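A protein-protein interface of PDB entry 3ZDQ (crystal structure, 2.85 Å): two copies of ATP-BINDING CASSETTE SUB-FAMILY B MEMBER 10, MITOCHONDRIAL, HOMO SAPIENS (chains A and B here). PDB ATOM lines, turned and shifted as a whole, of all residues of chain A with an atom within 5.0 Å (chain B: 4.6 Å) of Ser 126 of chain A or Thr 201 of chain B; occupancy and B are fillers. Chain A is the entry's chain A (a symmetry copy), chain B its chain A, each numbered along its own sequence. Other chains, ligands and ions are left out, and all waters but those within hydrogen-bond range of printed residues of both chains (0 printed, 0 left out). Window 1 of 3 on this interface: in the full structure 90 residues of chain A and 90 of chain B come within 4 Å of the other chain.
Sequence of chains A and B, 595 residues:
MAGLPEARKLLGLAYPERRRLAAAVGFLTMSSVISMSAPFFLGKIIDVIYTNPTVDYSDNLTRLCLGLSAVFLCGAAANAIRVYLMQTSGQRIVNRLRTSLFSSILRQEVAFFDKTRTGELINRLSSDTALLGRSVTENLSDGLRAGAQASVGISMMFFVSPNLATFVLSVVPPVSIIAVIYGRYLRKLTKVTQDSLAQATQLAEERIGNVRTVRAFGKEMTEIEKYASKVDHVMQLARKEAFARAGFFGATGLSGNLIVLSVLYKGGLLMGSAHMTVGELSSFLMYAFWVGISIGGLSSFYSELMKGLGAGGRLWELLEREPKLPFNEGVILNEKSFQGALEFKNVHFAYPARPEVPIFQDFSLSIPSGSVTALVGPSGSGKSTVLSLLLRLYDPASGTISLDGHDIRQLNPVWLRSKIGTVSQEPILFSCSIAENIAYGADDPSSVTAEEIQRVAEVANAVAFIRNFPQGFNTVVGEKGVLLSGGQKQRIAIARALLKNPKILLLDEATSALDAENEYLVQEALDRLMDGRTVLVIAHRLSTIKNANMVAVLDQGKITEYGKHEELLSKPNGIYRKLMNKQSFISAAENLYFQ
Hydrophobic or aromatic side chains of chain A within 4 Å of the printed part of chain B: Ile 122 and Leu 125.
Of the 9 printed residues of chain B, 3 touch a printed residue of chain A.
Printed residues of chain B that touch a printed residue of chain A: Thr 201, Ala 204 and Glu 205.
Hydrophobic or aromatic side chains of chain B within 4 Å of the printed part of chain A: Ala 204.
Among the printed residues, 3 pairs touch across the chains.
Among the printed residues, no Asp or Glu carboxylate lies within 4 Å of a Lys or Arg side-chain nitrogen of the other chain.
Ile 122 of chain A touches Glu 205 of chain B.
CB of Ala 204 of chain B touches CD2 of Leu 125 of chain A, 3.6 Å away.
Thr 201 of chain B touches Ser 126 of chain A (CG2 to OG, 3.7 Å).
No position is printed for both chains.
Of the printed residues of chain B, Ile 122 of chain A touches Glu 205 (3.6 Å).
Of the printed residues of chain B, Ser 126 of chain A touches Thr 201 (3.7 Å).
Ser 127 of chain A touches none of the printed residues of chain B.
Of chain A, only Ser 126 (3.7 Å) comes within 4 Å of Thr 201 of chain B.
Of the printed residues of chain A, Ala 204 of chain B touches Leu 125.
Printed residues of chain A within 4 Å of Glu 205 of chain B: Ile 122 (3.6 Å).
O of Leu 125 of chain A is in hydrogen-bond range of OG1 of Thr 129 of chain A, at 2.7 Å.
The side-chain hydroxyl of Thr 129 of chain A sits at hydrogen-bond distance from the backbone carbonyl oxygen of Ser 126 of chain A (3.2 Å).
OG1 of Thr 201 of chain B is in hydrogen-bond range of O of Leu 197 of chain B (3.0 Å).
The side-chain hydroxyl of Ser 126 of chain A sits at hydrogen-bond distance from the backbone carbonyl oxygen of Ile 122 of chain A, 3.0 Å away.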
ATOM      1  N   ILE A 122      -4.060  32.490  -3.240  1.00  0.00           N
ATOM      2  CA  ILE A 122      -4.688  31.207  -2.903  1.00  0.00           C
ATOM      3  C   ILE A 122      -3.898  30.521  -1.765  1.00  0.00           C
ATOM      4  O   ILE A 122      -4.532  29.946  -0.886  1.00  0.00           O
ATOM      5  CB  ILE A 122      -4.874  30.328  -4.170  1.00  0.00           C
ATOM      6  CG1 ILE A 122      -5.996  30.914  -5.064  1.00  0.00           C
ATOM      7  CG2 ILE A 122      -5.147  28.852  -3.841  1.00  0.00           C
ATOM      8  CD1 ILE A 122      -7.388  31.116  -4.343  1.00  0.00           C
ATOM      9  N   ASN A 123      -2.561  30.663  -1.716  1.00  0.00           N
ATOM     10  CA  ASN A 123      -1.765  30.120  -0.611  1.00  0.00           C
ATOM     11  C   ASN A 123      -2.110  30.841   0.695  1.00  0.00           C
ATOM     12  O   ASN A 123      -2.163  30.202   1.753  1.00  0.00           O
ATOM     13  CB  ASN A 123      -0.260  30.199  -0.884  1.00  0.00           C
ATOM     14  CG  ASN A 123       0.249  29.184  -1.894  1.00  0.00           C
ATOM     15  OD1 ASN A 123      -0.281  28.069  -2.037  1.00  0.00           O
ATOM     16  ND2 ASN A 123       1.317  29.545  -2.600  1.00  0.00           N
ATOM     17  N   ARG A 124      -2.405  32.153   0.617  1.00  0.00           N
ATOM     18  CA  ARG A 124      -2.821  32.942   1.783  1.00  0.00           C
ATOM     19  C   ARG A 124      -4.224  32.524   2.245  1.00  0.00           C
ATOM     20  O   ARG A 124      -4.470  32.477   3.446  1.00  0.00           O
ATOM     21  CB  ARG A 124      -2.774  34.453   1.484  1.00  0.00           C
ATOM     22  CG  ARG A 124      -1.364  34.932   1.245  1.00  0.00           C
ATOM     23  CD  ARG A 124      -1.162  36.420   1.362  1.00  0.00           C
ATOM     24  NE  ARG A 124       0.183  36.756   0.888  1.00  0.00           N
ATOM     25  CZ  ARG A 124       0.801  37.915   1.088  1.00  0.00           C
ATOM     26  NH1 ARG A 124       0.197  38.890   1.757  1.00  0.00           N
ATOM     27  NH2 ARG A 124       2.034  38.101   0.638  1.00  0.00           N
ATOM     28  N   LEU A 125      -5.131  32.208   1.296  1.00  0.00           N
ATOM     29  CA  LEU A 125      -6.510  31.811   1.585  1.00  0.00           C
ATOM     30  C   LEU A 125      -6.603  30.359   2.057  1.00  0.00           C
ATOM     31  O   LEU A 125      -7.515  30.042   2.824  1.00  0.00           O
ATOM     32  CB  LEU A 125      -7.378  32.027   0.343  1.00  0.00           C
ATOM     33  CG  LEU A 125      -8.911  31.960   0.472  1.00  0.00           C
ATOM     34  CD1 LEU A 125      -9.476  33.154   1.216  1.00  0.00           C
ATOM     35  CD2 LEU A 125      -9.538  31.931  -0.882  1.00  0.00           C
ATOM     36  N   SER A 126      -5.666  29.490   1.623  1.00  0.00           N
ATOM     37  CA  SER A 126      -5.606  28.071   2.000  1.00  0.00           C
ATOM     38  C   SER A 126      -4.746  27.822   3.244  1.00  0.00           C
ATOM     39  O   SER A 126      -5.278  27.573   4.327  1.00  0.00           O
ATOM     40  CB  SER A 126      -5.055  27.227   0.853  1.00  0.00           C
ATOM     41  OG  SER A 126      -5.886  27.315  -0.291  1.00  0.00           O
ATOM     42  N   SER A 127      -3.414  27.873   3.068  1.00  0.00           N
ATOM     43  CA  SER A 127      -2.422  27.573   4.083  1.00  0.00           C
ATOM     44  C   SER A 127      -2.429  28.522   5.240  1.00  0.00           C
ATOM     45  O   SER A 127      -2.494  28.056   6.382  1.00  0.00           O
ATOM     46  CB  SER A 127      -1.022  27.557   3.478  1.00  0.00           C
ATOM     47  OG  SER A 127      -0.913  26.551   2.485  1.00  0.00           O
ATOM     48  N   ASP A 128      -2.306  29.836   4.969  1.00  0.00           N
ATOM     49  CA  ASP A 128      -2.145  30.841   6.014  1.00  0.00           C
ATOM     50  C   ASP A 128      -3.368  30.992   6.900  1.00  0.00           C
ATOM     51  O   ASP A 128      -3.186  31.205   8.096  1.00  0.00           O
ATOM     52  CB  ASP A 128      -1.689  32.188   5.436  1.00  0.00           C
ATOM     53  CG  ASP A 128      -0.307  32.161   4.779  1.00  0.00           C
ATOM     54  OD1 ASP A 128       0.512  31.274   5.133  1.00  0.00           O
ATOM     55  OD2 ASP A 128      -0.046  33.025   3.918  1.00  0.00           O
ATOM     56  N   THR A 129      -4.589  30.812   6.364  1.00  0.00           N
ATOM     57  CA  THR A 129      -5.822  30.871   7.165  1.00  0.00           C
ATOM     58  C   THR A 129      -5.873  29.656   8.103  1.00  0.00           C
ATOM     59  O   THR A 129      -6.331  29.790   9.240  1.00  0.00           O
ATOM     60  CB  THR A 129      -7.094  30.969   6.299  1.00  0.00           C
ATOM     61  OG1 THR A 129      -7.229  29.794   5.509  1.00  0.00           O
ATOM     62  CG2 THR A 129      -7.117  32.207   5.420  1.00  0.00           C
ATOM     63  N   ALA A 130      -5.378  28.485   7.633  1.00  0.00           N
ATOM     64  CA  ALA A 130      -5.331  27.249   8.417  1.00  0.00           C
ATOM     65  C   ALA A 130      -4.367  27.403   9.575  1.00  0.00           C
ATOM     66  O   ALA A 130      -4.738  27.085  10.703  1.00  0.00           O
ATOM     67  CB  ALA A 130      -4.927  26.076   7.541  1.00  0.00           C
ATOM     68  N   LEU B 197     -14.299  21.906   0.646  1.00  0.00           N
ATOM     69  CA  LEU B 197     -13.271  22.930   0.774  1.00  0.00           C
ATOM     70  C   LEU B 197     -12.496  23.107  -0.540  1.00  0.00           C
ATOM     71  O   LEU B 197     -12.101  24.230  -0.857  1.00  0.00           O
ATOM     72  CB  LEU B 197     -12.312  22.593   1.925  1.00  0.00           C
ATOM     73  CG  LEU B 197     -11.132  23.548   2.182  1.00  0.00           C
ATOM     74  CD1 LEU B 197     -11.598  24.988   2.426  1.00  0.00           C
ATOM     75  CD2 LEU B 197     -10.265  23.029   3.321  1.00  0.00           C
ATOM     76  N   ALA B 198     -12.282  22.011  -1.295  1.00  0.00           N
ATOM     77  CA  ALA B 198     -11.586  22.046  -2.583  1.00  0.00           C
ATOM     78  C   ALA B 198     -12.428  22.823  -3.602  1.00  0.00           C
ATOM     79  O   ALA B 198     -11.896  23.668  -4.329  1.00  0.00           O
ATOM     80  CB  ALA B 198     -11.312  20.631  -3.070  1.00  0.00           C
ATOM     81  N   GLN B 199     -13.756  22.589  -3.597  1.00  0.00           N
ATOM     82  CA  GLN B 199     -14.715  23.276  -4.467  1.00  0.00           C
ATOM     83  C   GLN B 199     -14.677  24.784  -4.241  1.00  0.00           C
ATOM     84  O   GLN B 199     -14.580  25.547  -5.192  1.00  0.00           O
ATOM     85  CB  GLN B 199     -16.134  22.757  -4.203  1.00  0.00           C
ATOM     86  CG  GLN B 199     -16.457  21.433  -4.862  1.00  0.00           C
ATOM     87  CD  GLN B 199     -17.934  21.347  -5.153  1.00  0.00           C
ATOM     88  OE1 GLN B 199     -18.779  21.357  -4.249  1.00  0.00           O
ATOM     89  NE2 GLN B 199     -18.277  21.301  -6.430  1.00  0.00           N
ATOM     90  N   ALA B 200     -14.737  25.200  -2.968  1.00  0.00           N
ATOM     91  CA  ALA B 200     -14.725  26.585  -2.535  1.00  0.00           C
ATOM     92  C   ALA B 200     -13.441  27.256  -2.946  1.00  0.00           C
ATOM     93  O   ALA B 200     -13.493  28.367  -3.466  1.00  0.00           O
ATOM     94  CB  ALA B 200     -14.904  26.665  -1.028  1.00  0.00           C
ATOM     95  N   THR B 201     -12.300  26.577  -2.769  1.00  0.00           N
ATOM     96  CA  THR B 201     -10.980  27.118  -3.113  1.00  0.00           C
ATOM     97  C   THR B 201     -10.818  27.248  -4.627  1.00  0.00           C
ATOM     98  O   THR B 201     -10.191  28.213  -5.079  1.00  0.00           O
ATOM     99  CB  THR B 201      -9.880  26.276  -2.469  1.00  0.00           C
ATOM    100  OG1 THR B 201     -10.058  26.395  -1.056  1.00  0.00           O
ATOM    101  CG2 THR B 201      -8.465  26.763  -2.833  1.00  0.00           C
ATOM    102  N   GLN B 202     -11.396  26.299  -5.402  1.00  0.00           N
ATOM    103  CA  GLN B 202     -11.326  26.349  -6.859  1.00  0.00           C
ATOM    104  C   GLN B 202     -12.121  27.569  -7.376  1.00  0.00           C
ATOM    105  O   GLN B 202     -11.590  28.351  -8.178  1.00  0.00           O
ATOM    106  CB  GLN B 202     -11.794  25.030  -7.490  1.00  0.00           C
ATOM    107  CG  GLN B 202     -11.412  24.883  -8.981  1.00  0.00           C
ATOM    108  CD  GLN B 202     -10.007  25.360  -9.338  1.00  0.00           C
ATOM    109  OE1 GLN B 202      -8.990  24.833  -8.850  1.00  0.00           O
ATOM    110  NE2 GLN B 202      -9.927  26.381 -10.197  1.00  0.00           N
ATOM    111  N   LEU B 203     -13.344  27.767  -6.845  1.00  0.00           N
ATOM    112  CA  LEU B 203     -14.204  28.915  -7.134  1.00  0.00           C
ATOM    113  C   LEU B 203     -13.422  30.221  -6.870  1.00  0.00           C
ATOM    114  O   LEU B 203     -13.353  31.079  -7.745  1.00  0.00           O
ATOM    115  CB  LEU B 203     -15.477  28.841  -6.251  1.00  0.00           C
ATOM    116  CG  LEU B 203     -16.373  30.070  -6.190  1.00  0.00           C
ATOM    117  CD1 LEU B 203     -17.215  30.161  -7.393  1.00  0.00           C
ATOM    118  CD2 LEU B 203     -17.281  30.013  -5.007  1.00  0.00           C
ATOM    119  N   ALA B 204     -12.806  30.335  -5.682  1.00  0.00           N
ATOM    120  CA  ALA B 204     -11.992  31.470  -5.253  1.00  0.00           C
ATOM    121  C   ALA B 204     -10.859  31.746  -6.260  1.00  0.00           C
ATOM    122  O   ALA B 204     -10.765  32.870  -6.773  1.00  0.00           O
ATOM    123  CB  ALA B 204     -11.432  31.203  -3.865  1.00  0.00           C
ATOM    124  N   GLU B 205     -10.084  30.693  -6.622  1.00  0.00           N
ATOM    125  CA  GLU B 205      -8.977  30.716  -7.590  1.00  0.00           C
ATOM    126  C   GLU B 205      -9.416  31.225  -8.975  1.00  0.00           C
ATOM    127  O   GLU B 205      -8.750  32.094  -9.552  1.00  0.00           O
ATOM    128  CB  GLU B 205      -8.344  29.321  -7.713  1.00  0.00           C
ATOM    129  CG  GLU B 205      -7.078  29.302  -8.551  1.00  0.00           C
ATOM    130  CD  GLU B 205      -6.005  28.309  -8.149  1.00  0.00           C
ATOM    131  OE1 GLU B 205      -6.345  27.141  -7.841  1.00  0.00           O
ATOM    132  OE2 GLU B 205      -4.813  28.692  -8.190  1.00  0.00           O
